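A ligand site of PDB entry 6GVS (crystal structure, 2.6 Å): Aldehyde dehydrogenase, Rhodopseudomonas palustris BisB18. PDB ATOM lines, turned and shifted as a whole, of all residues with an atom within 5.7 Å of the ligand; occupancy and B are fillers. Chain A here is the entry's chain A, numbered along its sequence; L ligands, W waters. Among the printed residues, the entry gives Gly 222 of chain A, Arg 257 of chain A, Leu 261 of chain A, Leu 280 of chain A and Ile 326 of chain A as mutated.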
ATOM      1  N   ILE A 192      32.356  20.559  -6.594  1.00  0.00           N
ATOM      2  CA  ILE A 192      30.975  20.121  -6.419  1.00  0.00           C
ATOM      3  C   ILE A 192      30.938  19.247  -5.185  1.00  0.00           C
ATOM      4  O   ILE A 192      31.563  18.178  -5.155  1.00  0.00           O
ATOM      5  CB  ILE A 192      30.467  19.364  -7.654  1.00  0.00           C
ATOM      6  CG1 ILE A 192      30.750  20.164  -8.925  1.00  0.00           C
ATOM      7  CG2 ILE A 192      28.982  19.066  -7.521  1.00  0.00           C
ATOM      8  CD1 ILE A 192      30.592  19.384 -10.199  1.00  0.00           C
ATOM      9  N   THR A 193      30.221  19.684  -4.155  1.00  0.00           N
ATOM     10  CA  THR A 193      30.248  19.016  -2.863  1.00  0.00           C
ATOM     11  C   THR A 193      29.003  18.148  -2.665  1.00  0.00           C
ATOM     12  O   THR A 193      27.975  18.351  -3.314  1.00  0.00           O
ATOM     13  CB  THR A 193      30.333  20.036  -1.724  1.00  0.00           C
ATOM     14  OG1 THR A 193      29.191  20.907  -1.760  1.00  0.00           O
ATOM     15  CG2 THR A 193      31.616  20.860  -1.861  1.00  0.00           C
ATOM     16  N   PRO A 194      29.087  17.163  -1.764  1.00  0.00           N
ATOM     17  CA  PRO A 194      27.956  16.254  -1.565  1.00  0.00           C
ATOM     18  C   PRO A 194      27.013  16.684  -0.451  1.00  0.00           C
ATOM     19  O   PRO A 194      27.254  17.687   0.224  1.00  0.00           O
ATOM     20  CB  PRO A 194      28.650  14.929  -1.226  1.00  0.00           C
ATOM     21  CG  PRO A 194      29.849  15.374  -0.443  1.00  0.00           C
ATOM     22  CD  PRO A 194      30.279  16.715  -1.026  1.00  0.00           C
ATOM     23  N   THR A 195      25.934  15.917  -0.254  1.00  0.00           N
ATOM     24  CA  THR A 195      25.012  16.183   0.837  1.00  0.00           C
ATOM     25  C   THR A 195      25.436  15.530   2.138  1.00  0.00           C
ATOM     26  O   THR A 195      25.001  15.964   3.215  1.00  0.00           O
ATOM     27  CB  THR A 195      23.607  15.671   0.490  1.00  0.00           C
ATOM     28  OG1 THR A 195      23.253  16.086  -0.829  1.00  0.00           O
ATOM     29  CG2 THR A 195      22.594  16.221   1.476  1.00  0.00           C
ATOM     30  N   THR A 196      26.253  14.480   2.078  1.00  0.00           N
ATOM     31  CA  THR A 196      26.643  13.766   3.297  1.00  0.00           C
ATOM     32  C   THR A 196      27.621  14.597   4.120  1.00  0.00           C
ATOM     33  O   THR A 196      27.469  14.713   5.341  1.00  0.00           O
ATOM     34  CB  THR A 196      27.241  12.411   2.933  1.00  0.00           C
ATOM     35  OG1 THR A 196      28.180  12.555   1.865  1.00  0.00           O
ATOM     36  CG2 THR A 196      26.148  11.443   2.513  1.00  0.00           C
ATOM     37  N   ASN A 197      28.631  15.177   3.473  1.00  0.00           N
ATOM     38  CA  ASN A 197      29.669  15.933   4.152  1.00  0.00           C
ATOM     39  C   ASN A 197      29.734  17.333   3.558  1.00  0.00           C
ATOM     40  O   ASN A 197      30.713  17.712   2.898  1.00  0.00           O
ATOM     41  CB  ASN A 197      31.016  15.214   4.043  1.00  0.00           C
ATOM     42  CG  ASN A 197      30.944  13.766   4.481  1.00  0.00           C
ATOM     43  OD1 ASN A 197      30.923  13.473   5.679  1.00  0.00           O
ATOM     44  ND2 ASN A 197      30.908  12.861   3.524  1.00  0.00           N
ATOM     45  N   SER A 219      29.844  24.787  -6.068  1.00  0.00           N
ATOM     46  CA  SER A 219      28.461  24.526  -6.428  1.00  0.00           C
ATOM     47  C   SER A 219      27.903  23.504  -5.439  1.00  0.00           C
ATOM     48  O   SER A 219      28.020  22.294  -5.678  1.00  0.00           O
ATOM     49  CB  SER A 219      28.343  24.014  -7.862  1.00  0.00           C
ATOM     50  OG  SER A 219      26.983  23.819  -8.212  1.00  0.00           O
ATOM     51  N   PRO A 220      27.322  23.933  -4.330  1.00  0.00           N
ATOM     52  CA  PRO A 220      26.926  22.994  -3.288  1.00  0.00           C
ATOM     53  C   PRO A 220      25.588  22.333  -3.593  1.00  0.00           C
ATOM     54  O   PRO A 220      24.835  22.750  -4.472  1.00  0.00           O
ATOM     55  CB  PRO A 220      26.820  23.860  -2.022  1.00  0.00           C
ATOM     56  CG  PRO A 220      26.965  25.298  -2.492  1.00  0.00           C
ATOM     57  CD  PRO A 220      26.913  25.308  -3.987  1.00  0.00           C
ATOM     58  N   HIS A 221      25.300  21.279  -2.837  1.00  0.00           N
ATOM     59  CA  HIS A 221      24.023  20.587  -2.941  1.00  0.00           C
ATOM     60  C   HIS A 221      22.895  21.480  -2.443  1.00  0.00           C
ATOM     61  O   HIS A 221      23.006  22.119  -1.403  1.00  0.00           O
ATOM     62  CB  HIS A 221      24.063  19.290  -2.135  1.00  0.00           C
ATOM     63  CG  HIS A 221      23.406  18.128  -2.821  1.00  0.00           C
ATOM     64  ND1 HIS A 221      22.060  17.857  -2.700  1.00  0.00           N
ATOM     65  CD2 HIS A 221      23.917  17.173  -3.624  1.00  0.00           C
ATOM     66  CE1 HIS A 221      21.772  16.778  -3.402  1.00  0.00           C
ATOM     67  NE2 HIS A 221      22.874  16.336  -3.970  1.00  0.00           N
ATOM     68  N   GLY A 222      21.799  21.510  -3.205  1.00  0.00           N
ATOM     69  CA  GLY A 222      20.657  22.303  -2.797  1.00  0.00           C
ATOM     70  C   GLY A 222      20.113  21.917  -1.440  1.00  0.00           C
ATOM     71  O   GLY A 222      19.591  22.759  -0.710  1.00  0.00           O
ATOM     72  N   ARG A 257      21.303  22.304  -9.645  1.00  0.00           N
ATOM     73  CA  ARG A 257      21.991  21.555 -10.665  1.00  0.00           C
ATOM     74  C   ARG A 257      22.244  22.353 -11.926  1.00  0.00           C
ATOM     75  O   ARG A 257      23.167  22.124 -12.619  1.00  0.00           O
ATOM     76  CB  ARG A 257      21.256  20.259 -10.917  1.00  0.00           C
ATOM     77  CG  ARG A 257      21.046  19.940 -12.349  1.00  0.00           C
ATOM     78  CD  ARG A 257      22.067  18.934 -12.761  1.00  0.00           C
ATOM     79  NE  ARG A 257      21.884  17.692 -12.076  1.00  0.00           N
ATOM     80  CZ  ARG A 257      21.680  16.563 -12.714  1.00  0.00           C
ATOM     81  NH1 ARG A 257      21.536  15.432 -12.067  1.00  0.00           N
ATOM     82  NH2 ARG A 257      21.611  16.585 -14.033  1.00  0.00           N
ATOM     83  N   THR A 260      25.514  24.006 -11.301  1.00  0.00           N
ATOM     84  CA  THR A 260      26.627  23.083 -11.492  1.00  0.00           C
ATOM     85  C   THR A 260      26.984  22.974 -12.966  1.00  0.00           C
ATOM     86  O   THR A 260      28.147  23.158 -13.353  1.00  0.00           O
ATOM     87  CB  THR A 260      26.269  21.716 -10.910  1.00  0.00           C
ATOM     88  OG1 THR A 260      26.148  21.824  -9.493  1.00  0.00           O
ATOM     89  CG2 THR A 260      27.334  20.684 -11.258  1.00  0.00           C
ATOM     90  N   LEU A 261      25.988  22.700 -13.809  1.00  0.00           N
ATOM     91  CA  LEU A 261      26.238  22.603 -15.251  1.00  0.00           C
ATOM     92  C   LEU A 261      26.843  23.895 -15.792  1.00  0.00           C
ATOM     93  O   LEU A 261      27.756  23.852 -16.627  1.00  0.00           O
ATOM     94  CB  LEU A 261      24.948  22.268 -15.978  1.00  0.00           C
ATOM     95  CG  LEU A 261      24.363  20.888 -15.680  1.00  0.00           C
ATOM     96  CD1 LEU A 261      23.047  20.702 -16.409  1.00  0.00           C
ATOM     97  CD2 LEU A 261      25.342  19.798 -16.078  1.00  0.00           C
ATOM     98  N   MET A 264      30.435  23.854 -14.905  1.00  0.00           N
ATOM     99  CA  MET A 264      31.139  22.874 -15.722  1.00  0.00           C
ATOM    100  C   MET A 264      31.384  23.387 -17.139  1.00  0.00           C
ATOM    101  O   MET A 264      32.304  22.908 -17.804  1.00  0.00           O
ATOM    102  CB  MET A 264      30.343  21.563 -15.800  1.00  0.00           C
ATOM    103  CG  MET A 264      30.063  20.922 -14.450  1.00  0.00           C
ATOM    104  SD  MET A 264      29.312  19.269 -14.512  1.00  0.00           S
ATOM    105  CE  MET A 264      28.757  19.171 -16.213  1.00  0.00           C
ATOM    106  N   THR A 275      32.885  15.605  -5.947  1.00  0.00           N
ATOM    107  CA  THR A 275      32.731  14.674  -4.829  1.00  0.00           C
ATOM    108  C   THR A 275      31.259  14.257  -4.791  1.00  0.00           C
ATOM    109  O   THR A 275      30.413  15.018  -4.316  1.00  0.00           O
ATOM    110  CB  THR A 275      33.174  15.325  -3.523  1.00  0.00           C
ATOM    111  OG1 THR A 275      34.481  15.886  -3.690  1.00  0.00           O
ATOM    112  CG2 THR A 275      33.232  14.295  -2.403  1.00  0.00           C
ATOM    113  N   GLY A 276      30.973  13.062  -5.295  1.00  0.00           N
ATOM    114  CA  GLY A 276      29.602  12.589  -5.345  1.00  0.00           C
ATOM    115  C   GLY A 276      29.451  11.207  -5.931  1.00  0.00           C
ATOM    116  O   GLY A 276      30.308  10.342  -5.753  1.00  0.00           O
ATOM    117  N   GLY A 277      28.337  10.977  -6.639  1.00  0.00           N
ATOM    118  CA  GLY A 277      28.049   9.682  -7.183  1.00  0.00           C
ATOM    119  C   GLY A 277      28.733   9.442  -8.508  1.00  0.00           C
ATOM    120  O   GLY A 277      29.388  10.322  -9.077  1.00  0.00           O
ATOM    121  N   PRO A 278      28.584   8.219  -9.017  1.00  0.00           N
ATOM    122  CA  PRO A 278      29.189   7.896 -10.314  1.00  0.00           C
ATOM    123  C   PRO A 278      28.617   8.709 -11.469  1.00  0.00           C
ATOM    124  O   PRO A 278      29.352   8.997 -12.428  1.00  0.00           O
ATOM    125  CB  PRO A 278      28.890   6.397 -10.480  1.00  0.00           C
ATOM    126  CG  PRO A 278      27.693   6.150  -9.611  1.00  0.00           C
ATOM    127  CD  PRO A 278      27.859   7.071  -8.432  1.00  0.00           C
ATOM    128  N   ALA A 279      27.339   9.078 -11.409  1.00  0.00           N
ATOM    129  CA  ALA A 279      26.767   9.899 -12.472  1.00  0.00           C
ATOM    130  C   ALA A 279      27.445  11.263 -12.534  1.00  0.00           C
ATOM    131  O   ALA A 279      27.675  11.798 -13.629  1.00  0.00           O
ATOM    132  CB  ALA A 279      25.262  10.048 -12.269  1.00  0.00           C
ATOM    133  N   LEU A 280      27.745  11.848 -11.370  1.00  0.00           N
ATOM    134  CA  LEU A 280      28.446  13.128 -11.353  1.00  0.00           C
ATOM    135  C   LEU A 280      29.857  12.999 -11.892  1.00  0.00           C
ATOM    136  O   LEU A 280      30.312  13.844 -12.673  1.00  0.00           O
ATOM    137  CB  LEU A 280      28.459  13.691  -9.932  1.00  0.00           C
ATOM    138  CG  LEU A 280      29.392  14.887  -9.707  1.00  0.00           C
ATOM    139  CD1 LEU A 280      28.911  16.104 -10.479  1.00  0.00           C
ATOM    140  CD2 LEU A 280      29.535  15.200  -8.219  1.00  0.00           C
ATOM    141  N   ALA A 283      30.001  13.047 -15.523  1.00  0.00           N
ATOM    142  CA  ALA A 283      29.615  14.322 -16.126  1.00  0.00           C
ATOM    143  C   ALA A 283      30.801  15.273 -16.234  1.00  0.00           C
ATOM    144  O   ALA A 283      31.027  15.877 -17.285  1.00  0.00           O
ATOM    145  CB  ALA A 283      28.487  14.952 -15.317  1.00  0.00           C
ATOM    146  N   ALA A 294      35.832  11.968  -7.431  1.00  0.00           N
ATOM    147  CA  ALA A 294      35.751  11.167  -6.214  1.00  0.00           C
ATOM    148  C   ALA A 294      34.376  10.492  -6.198  1.00  0.00           C
ATOM    149  O   ALA A 294      33.387  11.096  -5.760  1.00  0.00           O
ATOM    150  CB  ALA A 294      35.976  12.036  -4.973  1.00  0.00           C
ATOM    151  N   GLY A 295      34.331   9.247  -6.664  1.00  0.00           N
ATOM    152  CA  GLY A 295      33.088   8.526  -6.801  1.00  0.00           C
ATOM    153  C   GLY A 295      32.654   7.834  -5.530  1.00  0.00           C
ATOM    154  O   GLY A 295      33.100   8.149  -4.422  1.00  0.00           O
ATOM    155  N   ALA A 296      31.750   6.865  -5.689  1.00  0.00           N
ATOM    156  CA  ALA A 296      31.166   6.164  -4.563  1.00  0.00           C
ATOM    157  C   ALA A 296      31.886   4.829  -4.358  1.00  0.00           C
ATOM    158  O   ALA A 296      32.761   4.435  -5.125  1.00  0.00           O
ATOM    159  CB  ALA A 296      29.668   5.957  -4.787  1.00  0.00           C
ATOM    160  N   GLY A 297      31.485   4.126  -3.302  1.00  0.00           N
ATOM    161  CA  GLY A 297      32.018   2.812  -2.998  1.00  0.00           C
ATOM    162  C   GLY A 297      30.979   1.937  -2.327  1.00  0.00           C
ATOM    163  O   GLY A 297      29.829   2.335  -2.130  1.00  0.00           O
ATOM    164  N   ILE A 326      27.358   7.465   6.696  1.00  0.00           N
ATOM    165  CA  ILE A 326      27.292   8.284   5.496  1.00  0.00           C
ATOM    166  C   ILE A 326      28.671   8.673   4.953  1.00  0.00           C
ATOM    167  O   ILE A 326      28.750   9.378   3.942  1.00  0.00           O
ATOM    168  CB  ILE A 326      26.470   9.570   5.715  1.00  0.00           C
ATOM    169  CG1 ILE A 326      27.175  10.521   6.687  1.00  0.00           C
ATOM    170  CG2 ILE A 326      25.079   9.223   6.230  1.00  0.00           C
ATOM    171  CD1 ILE A 326      26.417  11.826   6.909  1.00  0.00           C
ATOM    172  N   CYS A 328      31.965   7.869   2.874  1.00  0.00           N
ATOM    173  CA  CYS A 328      32.180   7.012   1.713  1.00  0.00           C
ATOM    174  C   CYS A 328      33.071   5.816   2.004  1.00  0.00           C
ATOM    175  O   CYS A 328      33.168   4.922   1.154  1.00  0.00           O
ATOM    176  CB  CYS A 328      32.781   7.837   0.572  1.00  0.00           C
ATOM    177  SG  CYS A 328      34.157   8.907   1.070  1.00  0.00           S
ATOM    178  N   GLU A 417      24.690   0.530  -1.747  1.00  0.00           N
ATOM    179  CA  GLU A 417      25.358   1.450  -0.836  1.00  0.00           C
ATOM    180  C   GLU A 417      24.283   2.182  -0.051  1.00  0.00           C
ATOM    181  O   GLU A 417      23.871   3.304  -0.367  1.00  0.00           O
ATOM    182  CB  GLU A 417      26.265   2.408  -1.600  1.00  0.00           C
ATOM    183  CG  GLU A 417      27.009   3.413  -0.727  1.00  0.00           C
ATOM    184  CD  GLU A 417      27.762   4.467  -1.538  1.00  0.00           C
ATOM    185  OE1 GLU A 417      27.206   4.951  -2.550  1.00  0.00           O
ATOM    186  OE2 GLU A 417      28.899   4.812  -1.149  1.00  0.00           O
ATOM    187  N   MET A 419      24.283   3.530   2.888  1.00  0.00           N
ATOM    188  CA  MET A 419      24.697   4.690   3.665  1.00  0.00           C
ATOM    189  C   MET A 419      23.826   4.826   4.921  1.00  0.00           C
ATOM    190  O   MET A 419      23.395   5.913   5.300  1.00  0.00           O
ATOM    191  CB  MET A 419      24.644   5.974   2.839  1.00  0.00           C
ATOM    192  CG  MET A 419      25.380   5.877   1.512  1.00  0.00           C
ATOM    193  SD  MET A 419      25.590   7.490   0.726  1.00  0.00           S
ATOM    194  CE  MET A 419      27.057   8.074   1.580  1.00  0.00           C
ATOM    195  N   HIS A 447      37.500   1.788  -4.253  1.00  0.00           N
ATOM    196  CA  HIS A 447      37.366   2.846  -3.265  1.00  0.00           C
ATOM    197  C   HIS A 447      37.960   2.426  -1.916  1.00  0.00           C
ATOM    198  O   HIS A 447      39.085   2.808  -1.600  1.00  0.00           O
ATOM    199  CB  HIS A 447      35.895   3.236  -3.093  1.00  0.00           C
ATOM    200  CG  HIS A 447      35.698   4.517  -2.359  1.00  0.00           C
ATOM    201  ND1 HIS A 447      36.117   4.704  -1.056  1.00  0.00           N
ATOM    202  CD2 HIS A 447      35.129   5.685  -2.747  1.00  0.00           C
ATOM    203  CE1 HIS A 447      35.812   5.939  -0.672  1.00  0.00           C
ATOM    204  NE2 HIS A 447      35.218   6.554  -1.676  1.00  0.00           N
ATOM    205  N   PHE A 491      38.488  14.645   2.465  1.00  0.00           N
ATOM    206  CA  PHE A 491      37.098  14.263   2.216  1.00  0.00           C
ATOM    207  C   PHE A 491      36.785  14.227   0.729  1.00  0.00           C
ATOM    208  O   PHE A 491      35.609  14.239   0.347  1.00  0.00           O
ATOM    209  CB  PHE A 491      36.141  15.208   2.952  1.00  0.00           C
ATOM    210  CG  PHE A 491      36.189  15.071   4.445  1.00  0.00           C
ATOM    211  CD1 PHE A 491      35.435  14.097   5.081  1.00  0.00           C
ATOM    212  CD2 PHE A 491      36.997  15.898   5.199  1.00  0.00           C
ATOM    213  CE1 PHE A 491      35.482  13.958   6.451  1.00  0.00           C
ATOM    214  CE2 PHE A 491      37.048  15.756   6.579  1.00  0.00           C
ATOM    215  CZ  PHE A 491      36.294  14.795   7.206  1.00  0.00           C
ATOM    216  N   THR A 492      37.811  14.167  -0.120  1.00  0.00           N
ATOM    217  CA  THR A 492      37.662  13.933  -1.550  1.00  0.00           C
ATOM    218  C   THR A 492      38.623  12.813  -1.917  1.00  0.00           C
ATOM    219  O   THR A 492      39.824  13.055  -2.136  1.00  0.00           O
ATOM    220  CB  THR A 492      37.923  15.208  -2.354  1.00  0.00           C
ATOM    221  OG1 THR A 492      36.908  16.175  -2.055  1.00  0.00           O
ATOM    222  CG2 THR A 492      37.916  14.900  -3.848  1.00  0.00           C
ATOM    223  N   ILE A 493      38.109  11.592  -1.987  1.00  0.00           N
ATOM    224  CA  ILE A 493      38.908  10.394  -2.238  1.00  0.00           C
ATOM    225  C   ILE A 493      38.665   9.995  -3.691  1.00  0.00           C
ATOM    226  O   ILE A 493      37.587   9.527  -4.050  1.00  0.00           O
ATOM    227  CB  ILE A 493      38.539   9.262  -1.263  1.00  0.00           C
ATOM    228  CG1 ILE A 493      38.766   9.746   0.176  1.00  0.00           C
ATOM    229  CG2 ILE A 493      39.358   8.011  -1.560  1.00  0.00           C
ATOM    230  CD1 ILE A 493      38.342   8.760   1.236  1.00  0.00           C
ATOM    231  N   ALA A 494      39.686  10.170  -4.526  1.00  0.00           N
ATOM    232  CA  ALA A 494      39.568   9.993  -5.973  1.00  0.00           C
ATOM    233  C   ALA A 494      40.092   8.627  -6.368  1.00  0.00           C
ATOM    234  O   ALA A 494      41.304   8.427  -6.530  1.00  0.00           O
ATOM    235  CB  ALA A 494      40.318  11.111  -6.709  1.00  0.00           C
HETATM  236  P1  LIG L   1      25.380  13.049  -5.716  1.00  0.00           P
HETATM  237  O1  LIG L   1      24.097  12.361  -5.762  1.00  0.00           O
HETATM  238  O2  LIG L   1      26.165  12.590  -6.834  1.00  0.00           O
HETATM  239  O3  LIG L   1      25.166  14.622  -5.866  1.00  0.00           O
HETATM  240  C1  LIG L   1      26.194  15.538  -5.725  1.00  0.00           C
HETATM  241  C2  LIG L   1      26.119  16.683  -6.783  1.00  0.00           C
HETATM  242  O4  LIG L   1      26.231  16.166  -7.961  1.00  0.00           O
HETATM  243  C3  LIG L   1      24.775  17.417  -6.848  1.00  0.00           C
HETATM  244  O5  LIG L   1      24.927  18.726  -7.124  1.00  0.00           O
HETATM  245  C4  LIG L   1      24.133  16.756  -8.037  1.00  0.00           C
HETATM  246  O6  LIG L   1      22.936  17.532  -8.378  1.00  0.00           O
HETATM  247  C5  LIG L   1      25.106  16.771  -8.900  1.00  0.00           C
HETATM  248  N1  LIG L   1      24.985  15.816  -9.961  1.00  0.00           N
HETATM  249  C6  LIG L   1      24.750  14.523  -9.948  1.00  0.00           C
HETATM  250  N2  LIG L   1      24.723  14.087 -11.183  1.00  0.00           N
HETATM  251  C7  LIG L   1      24.959  15.100 -11.976  1.00  0.00           C
HETATM  252  C8  LIG L   1      25.036  15.191 -13.319  1.00  0.00           C
HETATM  253  N3  LIG L   1      24.890  14.155 -14.284  1.00  0.00           N
HETATM  254  N4  LIG L   1      25.260  16.314 -13.888  1.00  0.00           N
HETATM  255  C9  LIG L   1      25.434  17.398 -13.163  1.00  0.00           C
HETATM  256  N5  LIG L   1      25.348  17.333 -11.831  1.00  0.00           N
HETATM  257  C10 LIG L   1      25.112  16.168 -11.237  1.00  0.00           C
HETATM  258  O7  LIG L   1      26.051  12.661  -4.344  1.00  0.00           O
HETATM  259  P2  LIG L   1      25.299  12.852  -2.962  1.00  0.00           P
HETATM  260  O8  LIG L   1      23.884  12.630  -3.144  1.00  0.00           O
HETATM  261  O9  LIG L   1      25.417  14.165  -2.405  1.00  0.00           O
HETATM  262  O10 LIG L   1      25.768  11.750  -1.919  1.00  0.00           O
HETATM  263  C11 LIG L   1      27.057  11.308  -1.738  1.00  0.00           C
HETATM  264  C12 LIG L   1      27.447  10.348  -2.850  1.00  0.00           C
HETATM  265  O11 LIG L   1      28.643  10.669  -3.155  1.00  0.00           O
HETATM  266  C13 LIG L   1      27.568   8.921  -2.379  1.00  0.00           C
HETATM  267  O12 LIG L   1      27.485   8.123  -3.432  1.00  0.00           O
HETATM  268  C14 LIG L   1      28.957   8.863  -1.781  1.00  0.00           C
HETATM  269  O13 LIG L   1      29.462   7.489  -1.794  1.00  0.00           O
HETATM  270  C15 LIG L   1      29.662   9.597  -2.567  1.00  0.00           C
HETATM  271  N6  LIG L   1      30.716  10.270  -1.874  1.00  0.00           N
HETATM  272  C16 LIG L   1      31.968  10.065  -2.241  1.00  0.00           C
HETATM  273  C17 LIG L   1      32.992  10.666  -1.569  1.00  0.00           C
HETATM  274  C18 LIG L   1      34.441  10.460  -1.978  1.00  0.00           C
HETATM  275  O14 LIG L   1      35.264  11.157  -1.601  1.00  0.00           O
HETATM  276  N7  LIG L   1      34.860   9.393  -2.812  1.00  0.00           N
HETATM  277  C19 LIG L   1      32.737  11.476  -0.562  1.00  0.00           C
HETATM  278  C20 LIG L   1      31.480  11.692  -0.189  1.00  0.00           C
HETATM  279  C21 LIG L   1      30.462  11.068  -0.859  1.00  0.00           C
HETATM  280  P3  LIG L   1      21.597  16.936  -7.766  1.00  0.00           P
HETATM  281  O15 LIG L   1      21.745  15.495  -7.475  1.00  0.00           O
HETATM  282  O16 LIG L   1      21.288  17.719  -6.591  1.00  0.00           O
HETATM  283  O17 LIG L   1      20.514  17.069  -8.735  1.00  0.00           O
HETATM  284  O   HOH W   1      22.214  10.662  -1.619  1.00  0.00           O
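O of Gly 295 is in hydrogen-bond range of N7 of the ligand (2.7 Å).
O2 of the ligand is in hydrogen-bond range of N of Gly 277 (2.7 Å).
O13 of the ligand lies within hydrogen-bond range of OE2 of Glu 417, 2.8 Å away.
O9 of the ligand sits at hydrogen-bond distance from N of Thr 195.
An oxygen (O9) of the ligand is in hydrogen-bond range of the side-chain hydroxyl (OG1) of Thr 195.
The backbone NH (N) of Ile 493 lies within hydrogen-bond range of an oxygen (O14) of the ligand, 2.9 Å away.
O of Ile 493 sits at hydrogen-bond distance from N7 of the ligand, 3.0 Å away.
A ring nitrogen (NE2) of His 447 is in hydrogen-bond range of a nitrogen (N7) of the ligand (3.1 Å).
A ring nitrogen (NE2) of His 221 lies close to an oxygen (O16) of the ligand, 3.4 Å away.
The side-chain sulfur (SG) of Cys 328 sits close to an oxygen (O14) of the ligand (3.7 Å).
O17 of the ligand lies within salt-bridge range of NE of Arg 257 (3.7 Å).
The backbone NH (N) of Gly 297 is in hydrogen-bond range of the side-chain carboxylate (OE2) of Glu 417 (3.4 Å).
A ring nitrogen (ND1) of His 221 lies within hydrogen-bond range of the side-chain hydroxyl of Thr 195, 2.8 Å away.
O of Ala 294 sits at hydrogen-bond distance from N of Gly 276, 3.1 Å away.
A ring nitrogen (NE2) of His 447 lies close to the side-chain sulfur (SG) of Cys 328 (3.8 Å).
The side-chain hydroxyl (OG1) of Thr 275 sits at hydrogen-bond distance from the side-chain hydroxyl (OG1) of Thr 492, 2.9 Å away.
The backbone NH (N) of Thr 275 is in hydrogen-bond range of the backbone carbonyl oxygen (O) of Ile 192 (3.0 Å).
The side-chain hydroxyl of Thr 196 is in hydrogen-bond range of the side-chain amide nitrogen of Asn 197 (3.2 Å).
The side-chain hydroxyl (OG1) of Thr 260 is in hydrogen-bond range of the side-chain hydroxyl (OG) of Ser 219 (2.5 Å).
O of Gly 276 lies close to O11 of the ligand, 3.1 Å away.
Merely in contact with the ligand: Ala 296 (3.4 Å), Pro 194 (3.4 Å), Thr 275 (3.4 Å), Leu 280 (3.5 Å), Ala 294 (3.6 Å), Phe 491 (3.7 Å), Thr 492 (3.7 Å), Ala 279 (3.7 Å), Leu 261 (3.8 Å), Ala 283 (3.8 Å), Ile 192 (3.8 Å), Thr 196 (3.9 Å), Asn 197 (3.9 Å), Thr 260 (3.9 Å) and Met 419 (3.9 Å).
25 residues have an atom within 4 Å of the ligand: Ile 192, Pro 194, Thr 195, Thr 196, Asn 197, His 221, Arg 257, Thr 260, Leu 261, Thr 275, Gly 276, Gly 277, Ala 279, Leu 280, Ala 283, Ala 294, Gly 295, Ala 296, Cys 328, Glu 417, Met 419, His 447, Phe 491, Thr 492 and Ile 493.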
